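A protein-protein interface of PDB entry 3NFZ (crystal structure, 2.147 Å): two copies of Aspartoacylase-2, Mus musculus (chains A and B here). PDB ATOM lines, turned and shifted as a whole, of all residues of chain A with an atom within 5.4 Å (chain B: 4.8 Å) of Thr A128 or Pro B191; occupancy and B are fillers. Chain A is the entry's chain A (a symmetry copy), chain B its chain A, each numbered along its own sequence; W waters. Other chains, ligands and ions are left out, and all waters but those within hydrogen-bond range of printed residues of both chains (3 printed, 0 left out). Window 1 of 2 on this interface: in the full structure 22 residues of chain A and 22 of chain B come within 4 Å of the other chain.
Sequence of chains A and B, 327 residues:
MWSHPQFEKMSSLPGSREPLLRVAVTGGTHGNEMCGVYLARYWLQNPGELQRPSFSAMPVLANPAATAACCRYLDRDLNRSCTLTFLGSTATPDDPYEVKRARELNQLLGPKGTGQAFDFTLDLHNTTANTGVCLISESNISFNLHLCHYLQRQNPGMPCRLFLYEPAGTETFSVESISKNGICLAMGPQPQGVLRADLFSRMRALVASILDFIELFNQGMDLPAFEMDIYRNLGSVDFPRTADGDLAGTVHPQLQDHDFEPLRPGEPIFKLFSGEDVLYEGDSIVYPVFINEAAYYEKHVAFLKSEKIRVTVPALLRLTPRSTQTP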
ATOM      1  N   ASN A 126      -6.751  -7.769  28.454  1.00  0.00           N
ATOM      2  CA  ASN A 126      -5.821  -8.216  27.422  1.00  0.00           C
ATOM      3  C   ASN A 126      -4.852  -9.215  28.009  1.00  0.00           C
ATOM      4  O   ASN A 126      -4.640  -9.245  29.221  1.00  0.00           O
ATOM      5  CB  ASN A 126      -5.042  -7.042  26.833  1.00  0.00           C
ATOM      6  CG  ASN A 126      -5.925  -6.118  26.026  1.00  0.00           C
ATOM      7  OD1 ASN A 126      -6.150  -4.983  26.421  1.00  0.00           O
ATOM      8  ND2 ASN A 126      -6.443  -6.608  24.881  1.00  0.00           N
ATOM      9  N   THR A 127      -4.272 -10.036  27.145  1.00  0.00           N
ATOM     10  CA  THR A 127      -3.244 -10.971  27.553  1.00  0.00           C
ATOM     11  C   THR A 127      -2.111 -10.904  26.529  1.00  0.00           C
ATOM     12  O   THR A 127      -2.344 -10.564  25.357  1.00  0.00           O
ATOM     13  CB  THR A 127      -3.818 -12.419  27.666  1.00  0.00           C
ATOM     14  OG1 THR A 127      -2.752 -13.355  27.906  1.00  0.00           O
ATOM     15  CG2 THR A 127      -4.528 -12.810  26.376  1.00  0.00           C
ATOM     16  N   THR A 128      -0.883 -11.178  26.975  1.00  0.00           N
ATOM     17  CA  THR A 128       0.236 -11.339  26.054  1.00  0.00           C
ATOM     18  C   THR A 128       0.263 -12.743  25.446  1.00  0.00           C
ATOM     19  O   THR A 128       1.107 -13.035  24.606  1.00  0.00           O
ATOM     20  CB  THR A 128       1.621 -11.070  26.738  1.00  0.00           C
ATOM     21  OG1 THR A 128       1.856 -12.045  27.761  1.00  0.00           O
ATOM     22  CG2 THR A 128       1.670  -9.674  27.356  1.00  0.00           C
ATOM     23  N   ALA A 129      -0.632 -13.624  25.892  1.00  0.00           N
ATOM     24  CA  ALA A 129      -0.726 -14.963  25.302  1.00  0.00           C
ATOM     25  C   ALA A 129      -1.535 -14.881  24.012  1.00  0.00           C
ATOM     26  O   ALA A 129      -2.379 -13.999  23.863  1.00  0.00           O
ATOM     27  CB  ALA A 129      -1.389 -15.943  26.284  1.00  0.00           C
ATOM     28  N   ASN A 130      -1.279 -15.792  23.080  1.00  0.00           N
ATOM     29  CA  ASN A 130      -2.008 -15.816  21.818  1.00  0.00           C
ATOM     30  C   ASN A 130      -3.418 -16.433  21.919  1.00  0.00           C
ATOM     31  O   ASN A 130      -3.735 -17.410  21.237  1.00  0.00           O
ATOM     32  CB  ASN A 130      -1.196 -16.561  20.750  1.00  0.00           C
ATOM     33  CG  ASN A 130      -1.840 -16.463  19.374  1.00  0.00           C
ATOM     34  OD1 ASN A 130      -2.520 -15.484  19.081  1.00  0.00           O
ATOM     35  ND2 ASN A 130      -1.628 -17.473  18.526  1.00  0.00           N
ATOM     36  N   PRO A 189      -3.015 -11.869  21.258  1.00  0.00           N
ATOM     37  CA  PRO A 189      -1.954 -11.293  22.096  1.00  0.00           C
ATOM     38  C   PRO A 189      -1.785  -9.794  21.926  1.00  0.00           C
ATOM     39  O   PRO A 189      -1.935  -9.267  20.825  1.00  0.00           O
ATOM     40  CB  PRO A 189      -0.688 -12.022  21.610  1.00  0.00           C
ATOM     41  CG  PRO A 189      -0.952 -12.301  20.141  1.00  0.00           C
ATOM     42  CD  PRO A 189      -2.503 -12.361  19.966  1.00  0.00           C
ATOM     43  N   GLN A 190      -1.469  -9.119  23.025  1.00  0.00           N
ATOM     44  CA  GLN A 190      -1.125  -7.707  23.005  1.00  0.00           C
ATOM     45  C   GLN A 190      -0.120  -7.436  24.123  1.00  0.00           C
ATOM     46  O   GLN A 190      -0.363  -7.780  25.280  1.00  0.00           O
ATOM     47  CB  GLN A 190      -2.380  -6.817  23.183  1.00  0.00           C
ATOM     48  CG  GLN A 190      -2.106  -5.335  22.978  1.00  0.00           C
ATOM     49  CD  GLN A 190      -3.366  -4.468  22.996  1.00  0.00           C
ATOM     50  OE1 GLN A 190      -3.807  -3.977  21.952  1.00  0.00           O
ATOM     51  NE2 GLN A 190      -3.933  -4.267  24.179  1.00  0.00           N
ATOM     52  N   PRO A 191       1.023  -6.821  23.783  1.00  0.00           N
ATOM     53  CA  PRO A 191       1.955  -6.471  24.858  1.00  0.00           C
ATOM     54  C   PRO A 191       1.275  -5.523  25.848  1.00  0.00           C
ATOM     55  O   PRO A 191       0.468  -4.690  25.450  1.00  0.00           O
ATOM     56  CB  PRO A 191       3.097  -5.744  24.129  1.00  0.00           C
ATOM     57  CG  PRO A 191       2.975  -6.185  22.659  1.00  0.00           C
ATOM     58  CD  PRO A 191       1.479  -6.366  22.457  1.00  0.00           C
ATOM     59  N   GLN A 192       1.568  -5.668  27.129  1.00  0.00           N
ATOM     60  CA  GLN A 192       1.157  -4.657  28.088  1.00  0.00           C
ATOM     61  C   GLN A 192       1.675  -3.279  27.660  1.00  0.00           C
ATOM     62  O   GLN A 192       2.751  -3.162  27.071  1.00  0.00           O
ATOM     63  CB  GLN A 192       1.682  -5.011  29.477  1.00  0.00           C
ATOM     64  CG  GLN A 192       1.102  -6.322  30.032  1.00  0.00           C
ATOM     65  CD  GLN A 192       1.913  -6.846  31.219  1.00  0.00           C
ATOM     66  OE1 GLN A 192       3.144  -6.878  31.171  1.00  0.00           O
ATOM     67  NE2 GLN A 192       1.225  -7.266  32.274  1.00  0.00           N
ATOM     68  N   GLN A 256       4.575 -22.270  22.520  1.00  0.00           N
ATOM     69  CA  GLN A 256       4.379 -20.834  22.435  1.00  0.00           C
ATOM     70  C   GLN A 256       3.346 -20.505  21.361  1.00  0.00           C
ATOM     71  O   GLN A 256       3.437 -21.018  20.243  1.00  0.00           O
ATOM     72  CB  GLN A 256       5.721 -20.153  22.109  1.00  0.00           C
ATOM     73  CG  GLN A 256       5.647 -18.636  21.994  1.00  0.00           C
ATOM     74  CD  GLN A 256       5.304 -17.964  23.314  1.00  0.00           C
ATOM     75  OE1 GLN A 256       6.030 -18.108  24.311  1.00  0.00           O
ATOM     76  NE2 GLN A 256       4.189 -17.224  23.332  1.00  0.00           N
ATOM     77  N   ILE A 291      -0.799 -19.205  27.622  1.00  0.00           N
ATOM     78  CA  ILE A 291       0.588 -19.626  27.500  1.00  0.00           C
ATOM     79  C   ILE A 291       1.510 -18.409  27.475  1.00  0.00           C
ATOM     80  O   ILE A 291       1.427 -17.585  26.556  1.00  0.00           O
ATOM     81  CB  ILE A 291       0.794 -20.441  26.213  1.00  0.00           C
ATOM     82  CG1 ILE A 291      -0.156 -21.639  26.193  1.00  0.00           C
ATOM     83  CG2 ILE A 291       2.265 -20.886  26.080  1.00  0.00           C
ATOM     84  CD1 ILE A 291      -0.163 -22.433  24.884  1.00  0.00           C
ATOM     85  N   ASN A 292       2.378 -18.293  28.485  1.00  0.00           N
ATOM     86  CA  ASN A 292       3.382 -17.215  28.548  1.00  0.00           C
ATOM     87  C   ASN A 292       2.760 -15.811  28.679  1.00  0.00           C
ATOM     88  O   ASN A 292       3.036 -14.919  27.878  1.00  0.00           O
ATOM     89  CB  ASN A 292       4.365 -17.289  27.360  1.00  0.00           C
ATOM     90  CG  ASN A 292       5.797 -16.908  27.749  1.00  0.00           C
ATOM     91  OD1 ASN A 292       6.731 -17.027  26.943  1.00  0.00           O
ATOM     92  ND2 ASN A 292       5.976 -16.455  28.974  1.00  0.00           N
ATOM     93  N   GLU A 293       1.913 -15.648  29.695  1.00  0.00           N
ATOM     94  CA  GLU A 293       1.348 -14.358  30.085  1.00  0.00           C
ATOM     95  C   GLU A 293       2.309 -13.621  31.032  1.00  0.00           C
ATOM     96  O   GLU A 293       2.680 -14.161  32.075  1.00  0.00           O
ATOM     97  CB  GLU A 293      -0.006 -14.580  30.779  1.00  0.00           C
ATOM     98  CG  GLU A 293      -0.527 -13.356  31.572  1.00  0.00           C
ATOM     99  CD  GLU A 293      -0.627 -12.086  30.724  1.00  0.00           C
ATOM    100  OE1 GLU A 293      -1.147 -12.154  29.582  1.00  0.00           O
ATOM    101  OE2 GLU A 293      -0.190 -11.015  31.206  1.00  0.00           O
ATOM    102  N   ALA A 294       2.702 -12.397  30.672  1.00  0.00           N
ATOM    103  CA  ALA A 294       3.634 -11.596  31.483  1.00  0.00           C
ATOM    104  C   ALA A 294       3.252 -11.514  32.967  1.00  0.00           C
ATOM    105  O   ALA A 294       4.105 -11.663  33.856  1.00  0.00           O
ATOM    106  CB  ALA A 294       3.771 -10.174  30.904  1.00  0.00           C
ATOM    107  N   THR B 128       8.813  -4.118  21.737  1.00  0.00           N
ATOM    108  CA  THR B 128       7.503  -4.644  21.376  1.00  0.00           C
ATOM    109  C   THR B 128       7.165  -4.352  19.912  1.00  0.00           C
ATOM    110  O   THR B 128       6.122  -4.772  19.424  1.00  0.00           O
ATOM    111  CB  THR B 128       6.354  -4.065  22.273  1.00  0.00           C
ATOM    112  OG1 THR B 128       6.241  -2.653  22.067  1.00  0.00           O
ATOM    113  CG2 THR B 128       6.618  -4.337  23.752  1.00  0.00           C
ATOM    114  N   PRO B 189       9.482  -8.673  17.673  1.00  0.00           N
ATOM    115  CA  PRO B 189       8.719  -8.180  18.829  1.00  0.00           C
ATOM    116  C   PRO B 189       8.700  -9.139  20.006  1.00  0.00           C
ATOM    117  O   PRO B 189       8.658 -10.354  19.823  1.00  0.00           O
ATOM    118  CB  PRO B 189       7.296  -8.014  18.265  1.00  0.00           C
ATOM    119  CG  PRO B 189       7.181  -9.092  17.203  1.00  0.00           C
ATOM    120  CD  PRO B 189       8.631  -9.392  16.707  1.00  0.00           C
ATOM    121  N   GLN B 190       8.729  -8.578  21.209  1.00  0.00           N
ATOM    122  CA  GLN B 190       8.566  -9.345  22.433  1.00  0.00           C
ATOM    123  C   GLN B 190       7.883  -8.458  23.473  1.00  0.00           C
ATOM    124  O   GLN B 190       8.340  -7.347  23.745  1.00  0.00           O
ATOM    125  CB  GLN B 190       9.927  -9.852  22.968  1.00  0.00           C
ATOM    126  CG  GLN B 190       9.797 -10.818  24.138  1.00  0.00           C
ATOM    127  CD  GLN B 190      11.124 -11.443  24.569  1.00  0.00           C
ATOM    128  OE1 GLN B 190      11.373 -12.627  24.321  1.00  0.00           O
ATOM    129  NE2 GLN B 190      11.967 -10.656  25.227  1.00  0.00           N
ATOM    130  N   PRO B 191       6.777  -8.941  24.059  1.00  0.00           N
ATOM    131  CA  PRO B 191       6.166  -8.143  25.125  1.00  0.00           C
ATOM    132  C   PRO B 191       7.165  -7.948  26.267  1.00  0.00           C
ATOM    133  O   PRO B 191       7.955  -8.840  26.555  1.00  0.00           O
ATOM    134  CB  PRO B 191       4.985  -9.008  25.597  1.00  0.00           C
ATOM    135  CG  PRO B 191       4.713  -9.980  24.434  1.00  0.00           C
ATOM    136  CD  PRO B 191       6.089 -10.227  23.838  1.00  0.00           C
ATOM    137  N   GLN B 192       7.156  -6.781  26.890  1.00  0.00           N
ATOM    138  CA  GLN B 192       7.896  -6.613  28.129  1.00  0.00           C
ATOM    139  C   GLN B 192       7.467  -7.673  29.150  1.00  0.00           C
ATOM    140  O   GLN B 192       6.308  -8.089  29.182  1.00  0.00           O
ATOM    141  CB  GLN B 192       7.663  -5.213  28.690  1.00  0.00           C
ATOM    142  CG  GLN B 192       8.189  -4.095  27.777  1.00  0.00           C
ATOM    143  CD  GLN B 192       7.614  -2.729  28.158  1.00  0.00           C
ATOM    144  OE1 GLN B 192       6.409  -2.600  28.388  1.00  0.00           O
ATOM    145  NE2 GLN B 192       8.467  -1.715  28.213  1.00  0.00           N
ATOM    146  N   GLY B 193       8.409  -8.113  29.982  1.00  0.00           N
ATOM    147  CA  GLY B 193       8.115  -9.103  31.008  1.00  0.00           C
ATOM    148  C   GLY B 193       7.806 -10.497  30.467  1.00  0.00           C
ATOM    149  O   GLY B 193       7.420 -11.381  31.220  1.00  0.00           O
ATOM    150  N   VAL B 194       7.961 -10.701  29.162  1.00  0.00           N
ATOM    151  CA  VAL B 194       7.786 -12.040  28.593  1.00  0.00           C
ATOM    152  C   VAL B 194       9.103 -12.519  28.007  1.00  0.00           C
ATOM    153  O   VAL B 194       9.775 -11.765  27.299  1.00  0.00           O
ATOM    154  CB  VAL B 194       6.700 -12.068  27.486  1.00  0.00           C
ATOM    155  CG1 VAL B 194       6.696 -13.408  26.777  1.00  0.00           C
ATOM    156  CG2 VAL B 194       5.309 -11.759  28.068  1.00  0.00           C
ATOM    157  N   ARG B 196      10.440 -15.159  25.389  1.00  0.00           N
ATOM    158  CA  ARG B 196      10.169 -16.146  24.344  1.00  0.00           C
ATOM    159  C   ARG B 196      11.423 -17.001  24.069  1.00  0.00           C
ATOM    160  O   ARG B 196      12.528 -16.475  23.971  1.00  0.00           O
ATOM    161  CB  ARG B 196       9.731 -15.460  23.053  1.00  0.00           C
ATOM    162  CG  ARG B 196       8.428 -14.671  23.155  1.00  0.00           C
ATOM    163  CD  ARG B 196       8.093 -14.020  21.812  1.00  0.00           C
ATOM    164  NE  ARG B 196       7.981 -15.014  20.748  1.00  0.00           N
ATOM    165  CZ  ARG B 196       6.834 -15.534  20.313  1.00  0.00           C
ATOM    166  NH1 ARG B 196       5.666 -15.154  20.838  1.00  0.00           N
ATOM    167  NH2 ARG B 196       6.854 -16.439  19.346  1.00  0.00           N
HETATM  168  O   HOH W   1       3.832  -7.041  28.246  1.00  0.00           O
HETATM  169  O   HOH W   2       5.056  -4.819  26.871  1.00  0.00           O
HETATM  170  O   HOH W   3       6.670 -10.929  33.895  1.00  0.00           O
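Of chain B, only Pro B191 (3.8 Å) and Val B194 (3.5 Å) come within 4 Å of Thr A128. Of chain A, only Thr A128 (3.8 Å) comes within 4 Å of Pro B191. Of the printed residues of chain A, Gly B193 touches Ala A294 (3.8 Å). Printed residues of chain B within 4 Å of Ala A294: Gln B192 (3.7 Å), Gly B193 (3.8 Å) and Val B194 (3.6 Å). Printed residues of chain B within 4 Å of Pro A191: Thr B128. Of the printed residues of chain A, Arg B196 touches Gln A256 (3.6 Å). The nearest residue of chain A that does not touch Pro B191 is Pro A191 (4.02 Å).
Water W3 lies within hydrogen-bond range of the backbone carbonyl oxygen (O) of Ala A294 (2.7 Å) and the backbone carbonyl oxygen (O) of Gly B193 (2.8 Å). Water W2 lies within hydrogen-bond range of O of Gln A192 and N of Gln B192. Water W1 bridges O of Gln B192 (2.8 Å) and N of Gln A192 (2.9 Å).
Of the 14 printed residues of chain A, 6 touch a printed residue of chain B.
Among the printed residues, merely in contact across the chains: Thr A128 with Val B194 (3.5 Å), Gln A256 with Arg B196 (3.6 Å), Ala A294 with Val B194 (3.6 Å), Asn A292 with Val B194 (3.6 Å), Ala A294 with Gln B192 (3.7 Å), Ala A294 with Gly B193 (3.8 Å), Pro A191 with Thr B128 (3.8 Å), Thr A128 with Pro B191 (3.8 Å) and Gln A192 with Gln B192 (3.9 Å).
Thr A128 touches Pro B191, and with the chains exchanged Pro A191 touches Thr B128. Gln A192 touches its own counterpart, Gln B192. Of the 9 pairs that touch across the chains among the printed residues, 3 have their exchanged pair printed and touching as well.
O of Val B194 lies close to NE2 of Gln B190 (3.2 Å). The backbone NH (N) of Arg B196 sits at hydrogen-bond distance from the side-chain amide oxygen (OE1) of Gln B190. The side-chain hydroxyl (OG1) of Thr A128 lies within hydrogen-bond range of the backbone carbonyl oxygen (O) of Asn A292, at 3.1 Å. The side-chain carboxylate (OE1) of Glu A293 lies within hydrogen-bond range of the backbone NH (N) of Thr A128 (2.8 Å). The side-chain hydroxyl (OG1) of Thr A128 sits at hydrogen-bond distance from the backbone NH (N) of Ala A294 (3.1 Å). The side-chain amide oxygen of Asn A292 sits close to the side-chain amide oxygen of Gln A256, at 2.9 Å.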
